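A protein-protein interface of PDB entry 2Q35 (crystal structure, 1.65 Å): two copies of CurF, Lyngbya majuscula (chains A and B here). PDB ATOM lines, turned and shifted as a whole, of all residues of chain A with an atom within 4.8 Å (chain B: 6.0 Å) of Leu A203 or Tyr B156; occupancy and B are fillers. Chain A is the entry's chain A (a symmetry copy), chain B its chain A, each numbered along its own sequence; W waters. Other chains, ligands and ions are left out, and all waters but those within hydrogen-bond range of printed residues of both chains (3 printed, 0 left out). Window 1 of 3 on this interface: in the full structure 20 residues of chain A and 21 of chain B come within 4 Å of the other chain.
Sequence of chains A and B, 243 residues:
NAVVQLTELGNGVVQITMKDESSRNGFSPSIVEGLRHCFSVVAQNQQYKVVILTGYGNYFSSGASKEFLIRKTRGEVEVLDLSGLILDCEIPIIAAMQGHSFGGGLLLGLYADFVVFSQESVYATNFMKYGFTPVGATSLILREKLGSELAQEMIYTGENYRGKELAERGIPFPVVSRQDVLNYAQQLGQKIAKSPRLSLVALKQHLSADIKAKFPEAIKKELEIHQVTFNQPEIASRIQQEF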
ATOM      1  N   PRO A  92      -6.427  20.128  -5.973  1.00  0.00           N
ATOM      2  CA  PRO A  92      -6.295  19.849  -7.416  1.00  0.00           C
ATOM      3  C   PRO A  92      -7.106  20.792  -8.310  1.00  0.00           C
ATOM      4  O   PRO A  92      -8.232  21.198  -7.962  1.00  0.00           O
ATOM      5  CB  PRO A  92      -6.865  18.428  -7.573  1.00  0.00           C
ATOM      6  CG  PRO A  92      -7.142  17.915  -6.237  1.00  0.00           C
ATOM      7  CD  PRO A  92      -6.883  18.965  -5.192  1.00  0.00           C
ATOM      8  N   ASP A 113      -3.381  20.484 -12.662  1.00  0.00           N
ATOM      9  CA  ASP A 113      -3.071  19.088 -12.409  1.00  0.00           C
ATOM     10  C   ASP A 113      -3.635  18.165 -13.468  1.00  0.00           C
ATOM     11  O   ASP A 113      -3.040  17.125 -13.787  1.00  0.00           O
ATOM     12  CB  ASP A 113      -3.573  18.705 -11.030  1.00  0.00           C
ATOM     13  CG  ASP A 113      -3.013  19.628  -9.966  1.00  0.00           C
ATOM     14  OD1 ASP A 113      -1.796  19.534  -9.645  1.00  0.00           O
ATOM     15  OD2 ASP A 113      -3.757  20.511  -9.514  1.00  0.00           O
ATOM     16  N   PHE A 114      -4.774  18.565 -14.019  1.00  0.00           N
ATOM     17  CA  PHE A 114      -5.430  17.847 -15.118  1.00  0.00           C
ATOM     18  C   PHE A 114      -5.826  18.862 -16.178  1.00  0.00           C
ATOM     19  O   PHE A 114      -6.066  20.032 -15.862  1.00  0.00           O
ATOM     20  CB  PHE A 114      -6.692  17.190 -14.590  1.00  0.00           C
ATOM     21  CG  PHE A 114      -6.422  16.120 -13.567  1.00  0.00           C
ATOM     22  CD1 PHE A 114      -6.399  16.437 -12.209  1.00  0.00           C
ATOM     23  CD2 PHE A 114      -6.181  14.813 -13.959  1.00  0.00           C
ATOM     24  CE1 PHE A 114      -6.136  15.452 -11.265  1.00  0.00           C
ATOM     25  CE2 PHE A 114      -5.945  13.820 -13.022  1.00  0.00           C
ATOM     26  CZ  PHE A 114      -5.893  14.150 -11.683  1.00  0.00           C
ATOM     27  N   ILE A 192     -12.715  12.862  -8.342  1.00  0.00           N
ATOM     28  CA  ILE A 192     -11.588  13.258  -7.469  1.00  0.00           C
ATOM     29  C   ILE A 192     -12.105  13.664  -6.087  1.00  0.00           C
ATOM     30  O   ILE A 192     -11.504  13.287  -5.055  1.00  0.00           O
ATOM     31  CB  ILE A 192     -10.759  14.358  -8.120  1.00  0.00           C
ATOM     32  CG1 ILE A 192     -10.061  13.808  -9.368  1.00  0.00           C
ATOM     33  CG2 ILE A 192      -9.686  14.895  -7.134  1.00  0.00           C
ATOM     34  CD1 ILE A 192      -9.365  14.906 -10.208  1.00  0.00           C
ATOM     35  N   SER A 195     -12.592  11.761  -2.393  1.00  0.00           N
ATOM     36  CA  SER A 195     -11.549  11.574  -1.375  1.00  0.00           C
ATOM     37  C   SER A 195     -11.600  12.661  -0.316  1.00  0.00           C
ATOM     38  O   SER A 195     -12.043  13.779  -0.592  1.00  0.00           O
ATOM     39  CB  SER A 195     -10.182  11.630  -2.040  1.00  0.00           C
ATOM     40  OG  SER A 195      -9.978  10.513  -2.882  1.00  0.00           O
ATOM     41  N   SER A 199      -6.356  14.202   2.300  1.00  0.00           N
ATOM     42  CA  SER A 199      -5.614  13.273   1.445  1.00  0.00           C
ATOM     43  C   SER A 199      -5.321  13.900   0.083  1.00  0.00           C
ATOM     44  O   SER A 199      -4.236  13.706  -0.488  1.00  0.00           O
ATOM     45  CB  SER A 199      -6.405  11.971   1.275  1.00  0.00           C
ATOM     46  OG  SER A 199      -6.529  11.285   2.515  1.00  0.00           O
ATOM     47  N   LEU A 200      -6.286  14.655  -0.441  1.00  0.00           N
ATOM     48  CA  LEU A 200      -6.075  15.354  -1.729  1.00  0.00           C
ATOM     49  C   LEU A 200      -4.921  16.357  -1.633  1.00  0.00           C
ATOM     50  O   LEU A 200      -4.057  16.409  -2.518  1.00  0.00           O
ATOM     51  CB  LEU A 200      -7.348  16.041  -2.194  1.00  0.00           C
ATOM     52  CG  LEU A 200      -8.471  15.082  -2.628  1.00  0.00           C
ATOM     53  CD1 LEU A 200      -9.758  15.923  -2.817  1.00  0.00           C
ATOM     54  CD2 LEU A 200      -8.097  14.354  -3.885  1.00  0.00           C
ATOM     55  N   VAL A 201      -4.905  17.136  -0.552  1.00  0.00           N
ATOM     56  CA  VAL A 201      -3.889  18.171  -0.352  1.00  0.00           C
ATOM     57  C   VAL A 201      -2.498  17.518  -0.210  1.00  0.00           C
ATOM     58  O   VAL A 201      -1.532  17.929  -0.878  1.00  0.00           O
ATOM     59  CB  VAL A 201      -4.238  19.061   0.856  1.00  0.00           C
ATOM     60  CG1 VAL A 201      -3.053  19.994   1.201  1.00  0.00           C
ATOM     61  CG2 VAL A 201      -5.503  19.855   0.560  1.00  0.00           C
ATOM     62  N   ALA A 202      -2.435  16.457   0.587  1.00  0.00           N
ATOM     63  CA  ALA A 202      -1.176  15.737   0.843  1.00  0.00           C
ATOM     64  C   ALA A 202      -0.640  15.087  -0.435  1.00  0.00           C
ATOM     65  O   ALA A 202       0.554  15.179  -0.764  1.00  0.00           O
ATOM     66  CB  ALA A 202      -1.370  14.719   1.921  1.00  0.00           C
ATOM     67  N   LEU A 203      -1.545  14.466  -1.194  1.00  0.00           N
ATOM     68  CA  LEU A 203      -1.141  13.818  -2.423  1.00  0.00           C
ATOM     69  C   LEU A 203      -0.629  14.839  -3.423  1.00  0.00           C
ATOM     70  O   LEU A 203       0.398  14.616  -4.053  1.00  0.00           O
ATOM     71  CB  LEU A 203      -2.341  13.042  -3.029  1.00  0.00           C
ATOM     72  CG  LEU A 203      -2.010  12.294  -4.320  1.00  0.00           C
ATOM     73  CD1 LEU A 203      -0.938  11.242  -4.097  1.00  0.00           C
ATOM     74  CD2 LEU A 203      -3.323  11.638  -4.894  1.00  0.00           C
ATOM     75  N   LYS A 204      -1.366  15.937  -3.601  1.00  0.00           N
ATOM     76  CA  LYS A 204      -0.982  16.946  -4.594  1.00  0.00           C
ATOM     77  C   LYS A 204       0.388  17.516  -4.261  1.00  0.00           C
ATOM     78  O   LYS A 204       1.231  17.706  -5.167  1.00  0.00           O
ATOM     79  CB  LYS A 204      -2.027  18.076  -4.676  1.00  0.00           C
ATOM     80  CG  LYS A 204      -1.580  19.160  -5.630  1.00  0.00           C
ATOM     81  CD  LYS A 204      -2.612  20.225  -5.846  1.00  0.00           C
ATOM     82  CE  LYS A 204      -1.987  21.418  -6.550  1.00  0.00           C
ATOM     83  NZ  LYS A 204      -2.994  22.156  -7.355  1.00  0.00           N
ATOM     84  N   GLN A 205       0.638  17.739  -2.971  1.00  0.00           N
ATOM     85  CA  GLN A 205       1.948  18.281  -2.555  1.00  0.00           C
ATOM     86  C   GLN A 205       3.075  17.299  -2.937  1.00  0.00           C
ATOM     87  O   GLN A 205       4.122  17.684  -3.486  1.00  0.00           O
ATOM     88  CB  GLN A 205       1.966  18.557  -1.060  1.00  0.00           C
ATOM     89  CG  GLN A 205       3.322  19.082  -0.604  1.00  0.00           C
ATOM     90  CD  GLN A 205       3.319  19.621   0.785  1.00  0.00           C
ATOM     91  OE1 GLN A 205       3.501  20.813   0.987  1.00  0.00           O
ATOM     92  NE2 GLN A 205       3.113  18.751   1.764  1.00  0.00           N
ATOM     93  N   HIS A 206       2.838  16.024  -2.652  1.00  0.00           N
ATOM     94  CA  HIS A 206       3.786  14.972  -2.989  1.00  0.00           C
ATOM     95  C   HIS A 206       4.034  14.875  -4.501  1.00  0.00           C
ATOM     96  O   HIS A 206       5.189  14.907  -4.944  1.00  0.00           O
ATOM     97  CB  HIS A 206       3.271  13.651  -2.419  1.00  0.00           C
ATOM     98  CG  HIS A 206       4.088  12.462  -2.823  1.00  0.00           C
ATOM     99  ND1 HIS A 206       5.336  12.209  -2.304  1.00  0.00           N
ATOM    100  CD2 HIS A 206       3.830  11.461  -3.698  1.00  0.00           C
ATOM    101  CE1 HIS A 206       5.824  11.105  -2.853  1.00  0.00           C
ATOM    102  NE2 HIS A 206       4.921  10.625  -3.691  1.00  0.00           N
ATOM    103  N   LEU A 207       2.957  14.804  -5.290  1.00  0.00           N
ATOM    104  CA  LEU A 207       3.077  14.660  -6.741  1.00  0.00           C
ATOM    105  C   LEU A 207       3.723  15.871  -7.428  1.00  0.00           C
ATOM    106  O   LEU A 207       4.358  15.726  -8.478  1.00  0.00           O
ATOM    107  CB  LEU A 207       1.705  14.396  -7.376  1.00  0.00           C
ATOM    108  CG  LEU A 207       1.068  13.064  -6.991  1.00  0.00           C
ATOM    109  CD1 LEU A 207      -0.360  12.962  -7.515  1.00  0.00           C
ATOM    110  CD2 LEU A 207       1.889  11.908  -7.534  1.00  0.00           C
ATOM    111  N   THR B 125      -4.937   1.586  -8.730  1.00  0.00           N
ATOM    112  CA  THR B 125      -4.143   2.002  -7.560  1.00  0.00           C
ATOM    113  C   THR B 125      -5.245   2.544  -6.656  1.00  0.00           C
ATOM    114  O   THR B 125      -5.628   3.718  -6.766  1.00  0.00           O
ATOM    115  CB  THR B 125      -3.135   3.131  -7.889  1.00  0.00           C
ATOM    116  OG1 THR B 125      -3.771   4.171  -8.640  1.00  0.00           O
ATOM    117  CG2 THR B 125      -1.931   2.629  -8.694  1.00  0.00           C
ATOM    118  N   MET B 128      -6.591   5.682  -2.809  1.00  0.00           N
ATOM    119  CA  MET B 128      -7.434   6.857  -2.590  1.00  0.00           C
ATOM    120  C   MET B 128      -8.933   6.548  -2.604  1.00  0.00           C
ATOM    121  O   MET B 128      -9.744   7.360  -2.134  1.00  0.00           O
ATOM    122  CB  MET B 128      -7.088   7.980  -3.572  1.00  0.00           C
ATOM    123  CG  MET B 128      -5.696   8.613  -3.311  1.00  0.00           C
ATOM    124  SD  MET B 128      -5.716   9.712  -1.882  1.00  0.00           S
ATOM    125  CE  MET B 128      -6.358  11.209  -2.620  1.00  0.00           C
ATOM    126  N   LYS B 129      -9.284   5.389  -3.148  1.00  0.00           N
ATOM    127  CA  LYS B 129     -10.672   4.913  -3.050  1.00  0.00           C
ATOM    128  C   LYS B 129     -11.042   4.701  -1.591  1.00  0.00           C
ATOM    129  O   LYS B 129     -12.141   5.067  -1.161  1.00  0.00           O
ATOM    130  CB  LYS B 129     -10.874   3.631  -3.837  1.00  0.00           C
ATOM    131  CG  LYS B 129     -12.303   3.040  -3.703  1.00  0.00           C
ATOM    132  CD  LYS B 129     -12.730   2.226  -4.918  1.00  0.00           C
ATOM    133  CE  LYS B 129     -13.505   3.069  -5.949  1.00  0.00           C
ATOM    134  NZ  LYS B 129     -13.807   2.353  -7.261  1.00  0.00           N
ATOM    135  N   THR B 133      -3.430   7.952   1.069  1.00  0.00           N
ATOM    136  CA  THR B 133      -2.416   8.107   0.010  1.00  0.00           C
ATOM    137  C   THR B 133      -1.610   6.816  -0.192  1.00  0.00           C
ATOM    138  O   THR B 133      -1.626   5.933   0.674  1.00  0.00           O
ATOM    139  CB  THR B 133      -1.468   9.274   0.336  1.00  0.00           C
ATOM    140  OG1 THR B 133      -0.904   9.050   1.633  1.00  0.00           O
ATOM    141  CG2 THR B 133      -2.242  10.602   0.379  1.00  0.00           C
ATOM    142  N   PRO B 134      -0.952   6.667  -1.357  1.00  0.00           N
ATOM    143  CA  PRO B 134      -0.264   5.401  -1.702  1.00  0.00           C
ATOM    144  C   PRO B 134       0.942   5.030  -0.837  1.00  0.00           C
ATOM    145  O   PRO B 134       1.456   5.852  -0.067  1.00  0.00           O
ATOM    146  CB  PRO B 134       0.209   5.630  -3.153  1.00  0.00           C
ATOM    147  CG  PRO B 134      -0.674   6.728  -3.665  1.00  0.00           C
ATOM    148  CD  PRO B 134      -0.946   7.630  -2.484  1.00  0.00           C
ATOM    149  N   ALA B 151      -0.853   8.077 -14.695  1.00  0.00           N
ATOM    150  CA  ALA B 151      -0.460   7.900 -13.306  1.00  0.00           C
ATOM    151  C   ALA B 151      -1.285   8.846 -12.423  1.00  0.00           C
ATOM    152  O   ALA B 151      -1.865   8.413 -11.431  1.00  0.00           O
ATOM    153  CB  ALA B 151       1.042   8.144 -13.134  1.00  0.00           C
ATOM    154  N   GLN B 152      -1.346  10.117 -12.810  1.00  0.00           N
ATOM    155  CA  GLN B 152      -2.106  11.146 -12.070  1.00  0.00           C
ATOM    156  C   GLN B 152      -3.568  10.727 -11.867  1.00  0.00           C
ATOM    157  O   GLN B 152      -4.112  10.735 -10.754  1.00  0.00           O
ATOM    158  CB  GLN B 152      -2.078  12.443 -12.886  1.00  0.00           C
ATOM    159  CG  GLN B 152      -2.440  13.678 -12.152  1.00  0.00           C
ATOM    160  CD  GLN B 152      -1.237  14.383 -11.573  1.00  0.00           C
ATOM    161  OE1 GLN B 152      -0.194  13.776 -11.331  1.00  0.00           O
ATOM    162  NE2 GLN B 152      -1.377  15.666 -11.347  1.00  0.00           N
ATOM    163  N   GLU B 153      -4.217  10.337 -12.946  1.00  0.00           N
ATOM    164  CA  GLU B 153      -5.646  10.067 -12.824  1.00  0.00           C
ATOM    165  C   GLU B 153      -5.923   8.802 -12.013  1.00  0.00           C
ATOM    166  O   GLU B 153      -6.836   8.788 -11.178  1.00  0.00           O
ATOM    167  CB  GLU B 153      -6.311   9.977 -14.188  1.00  0.00           C
ATOM    168  CG  GLU B 153      -7.832   9.934 -14.073  1.00  0.00           C
ATOM    169  CD  GLU B 153      -8.517   9.615 -15.390  1.00  0.00           C
ATOM    170  OE1 GLU B 153      -8.401  10.426 -16.326  1.00  0.00           O
ATOM    171  OE2 GLU B 153      -9.185   8.562 -15.489  1.00  0.00           O
ATOM    172  N   MET B 154      -5.153   7.749 -12.265  1.00  0.00           N
ATOM    173  CA  MET B 154      -5.352   6.503 -11.531  1.00  0.00           C
ATOM    174  C   MET B 154      -5.098   6.695 -10.030  1.00  0.00           C
ATOM    175  O   MET B 154      -5.843   6.195  -9.207  1.00  0.00           O
ATOM    176  CB  MET B 154      -4.454   5.382 -12.066  1.00  0.00           C
ATOM    177  CG  MET B 154      -4.797   4.962 -13.486  1.00  0.00           C
ATOM    178  SD  MET B 154      -3.793   3.585 -14.031  1.00  0.00           S
ATOM    179  CE  MET B 154      -4.477   2.269 -13.057  1.00  0.00           C
ATOM    180  N   ILE B 155      -4.070   7.464  -9.692  1.00  0.00           N
ATOM    181  CA  ILE B 155      -3.724   7.661  -8.269  1.00  0.00           C
ATOM    182  C   ILE B 155      -4.772   8.548  -7.577  1.00  0.00           C
ATOM    183  O   ILE B 155      -5.281   8.212  -6.506  1.00  0.00           O
ATOM    184  CB  ILE B 155      -2.299   8.249  -8.118  1.00  0.00           C
ATOM    185  CG1 ILE B 155      -1.271   7.247  -8.649  1.00  0.00           C
ATOM    186  CG2 ILE B 155      -1.975   8.562  -6.657  1.00  0.00           C
ATOM    187  CD1 ILE B 155       0.162   7.788  -8.707  1.00  0.00           C
ATOM    188  N   TYR B 156      -5.136   9.674  -8.191  1.00  0.00           N
ATOM    189  CA  TYR B 156      -6.143  10.537  -7.562  1.00  0.00           C
ATOM    190  C   TYR B 156      -7.517   9.915  -7.398  1.00  0.00           C
ATOM    191  O   TYR B 156      -8.170  10.149  -6.370  1.00  0.00           O
ATOM    192  CB  TYR B 156      -6.317  11.842  -8.330  1.00  0.00           C
ATOM    193  CG  TYR B 156      -5.400  12.981  -7.952  1.00  0.00           C
ATOM    194  CD1 TYR B 156      -5.728  13.839  -6.895  1.00  0.00           C
ATOM    195  CD2 TYR B 156      -4.249  13.245  -8.688  1.00  0.00           C
ATOM    196  CE1 TYR B 156      -4.898  14.944  -6.553  1.00  0.00           C
ATOM    197  CE2 TYR B 156      -3.426  14.341  -8.372  1.00  0.00           C
ATOM    198  CZ  TYR B 156      -3.761  15.183  -7.306  1.00  0.00           C
ATOM    199  OH  TYR B 156      -2.985  16.265  -6.973  1.00  0.00           O
ATOM    200  N   THR B 157      -7.995   9.192  -8.415  1.00  0.00           N
ATOM    201  CA  THR B 157      -9.363   8.660  -8.363  1.00  0.00           C
ATOM    202  C   THR B 157      -9.499   7.324  -7.614  1.00  0.00           C
ATOM    203  O   THR B 157     -10.575   7.020  -7.089  1.00  0.00           O
ATOM    204  CB  THR B 157     -10.002   8.469  -9.753  1.00  0.00           C
ATOM    205  OG1 THR B 157      -9.364   7.387 -10.438  1.00  0.00           O
ATOM    206  CG2 THR B 157      -9.970   9.753 -10.590  1.00  0.00           C
ATOM    207  N   GLY B 158      -8.448   6.519  -7.644  1.00  0.00           N
ATOM    208  CA  GLY B 158      -8.452   5.177  -7.062  1.00  0.00           C
ATOM    209  C   GLY B 158      -9.360   4.173  -7.778  1.00  0.00           C
ATOM    210  O   GLY B 158      -9.557   3.067  -7.276  1.00  0.00           O
ATOM    211  N   ILE B 225       3.646  10.050   4.519  1.00  0.00           N
ATOM    212  CA  ILE B 225       2.394  10.756   4.199  1.00  0.00           C
ATOM    213  C   ILE B 225       1.244   9.778   4.432  1.00  0.00           C
ATOM    214  O   ILE B 225       0.175  10.144   4.949  1.00  0.00           O
ATOM    215  CB  ILE B 225       2.407  11.256   2.720  1.00  0.00           C
ATOM    216  CG1 ILE B 225       3.550  12.254   2.511  1.00  0.00           C
ATOM    217  CG2 ILE B 225       1.047  11.877   2.317  1.00  0.00           C
ATOM    218  CD1 ILE B 225       3.975  12.396   1.050  1.00  0.00           C
HETATM  219  O   HOH W   1     -10.816  10.334  -5.232  1.00  0.00           O
HETATM  220  O   HOH W   2      -1.107  16.942  -8.830  1.00  0.00           O
HETATM  221  O   HOH W   3     -12.001   8.508  -3.101  1.00  0.00           O
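Leu A203 touches just these residues of chain B: Met B128, Pro B134, Ile B155 and Tyr B156. Of chain A, only Pro A92, Phe A114, Ser A195, Leu A200, Leu A203, Lys A204 and Leu A207 come within 4 Å of Tyr B156. Of the printed residues of chain B, Ser A199 touches Met B128 and Thr B133. Printed residues of chain A within 4 Å of Ile B155: Leu A203. Of the printed residues of chain B, Leu A200 touches Met B128 (3.8 Å) and Tyr B156 (3.9 Å). Of the printed residues of chain B, Ser A195 touches Met B128 and Tyr B156. Of the printed residues of chain A, Met B128 touches Ser A195 (3.2 Å), Ser A199 (3.9 Å), Leu A200 (3.8 Å) and Leu A203 (3.8 Å). The nearest residue of chain B that does not touch Leu A203 is Thr B133 (4.2 Å). The nearest residue of chain A that does not touch Tyr B156 is Ile A192 (4.1 Å).
N of Ile B155 sits at hydrogen-bond distance from OG1 of Thr B125 (3.5 Å). The backbone carbonyl oxygen of Glu B153 is in hydrogen-bond range of the side-chain hydroxyl of Thr B157, at 3.0 Å. The side-chain carboxylate (OD2) of Asp A113 lies within salt-bridge range of the side-chain amino group (NZ) of Lys A204 (2.8 Å).
O of Met B128 sits at hydrogen-bond distance from OG of Ser A195. O of Asp A113 is in hydrogen-bond range of NE2 of Gln B152 (3.3 Å).
Phe A114 touches Gln B152 (CZ to CG, 3.5 Å). Phe A114 touches Tyr B156 (CZ to CD2, 3.5 Å). Ser A199 touches Met B128. CG2 of Thr B133 touches O of Ser A199, 3.8 Å away. CD2 of Leu A200 touches CE of Met B128 (3.8 Å). CD of Pro B134 touches CD1 of Leu A203 (3.96 Å). Ile B155 touches Leu A203 (CG2 to CD2, 3.8 Å). ND1 of His A206 touches CD1 of Ile B225, 3.6 Å away. Gln B152 touches Leu A207. Leu A207 touches Tyr B156.
No position is printed for both chains.
Water W1 lies within hydrogen-bond range of OG of Ser A195 (2.5 Å), O of Tyr B156 (2.9 Å) and O of Ile A192 (3.0 Å). Water W3 lies within hydrogen-bond range of O of Met B128 (2.7 Å) and OG of Ser A195 (2.9 Å). Water W2 lies within hydrogen-bond range of OH of Tyr B156 (2.7 Å), OD1 of Asp A113 (2.8 Å) and NE2 of Gln B152 (2.8 Å).
Of the 14 printed residues of chain B, 8 touch a printed residue of chain A. Hydrophobic or aromatic side chains of chain B within 4 Å of the printed part of chain A: Met B128, Pro B134, Ile B155, Tyr B156 and Ile B225. Of the 14 printed residues of chain A, 11 touch a printed residue of chain B. Printed residues of chain A that touch a printed residue of chain B: Pro A92, Asp A113, Phe A114, Ser A195, Ser A199, Leu A200, Ala A202, Leu A203, Lys A204, His A206 and Leu A207. Hydrophobic or aromatic side chains of chain A within 4 Å of the printed part of chain B: Pro A92, Phe A114, Leu A200, Ala A202, Leu A203, His A206 and Leu A207. Among the printed residues, 20 pairs touch across the chains. Among the printed residues, no Asp or Glu carboxylate lies within 4 Å of a Lys or Arg side-chain nitrogen of the other chain.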
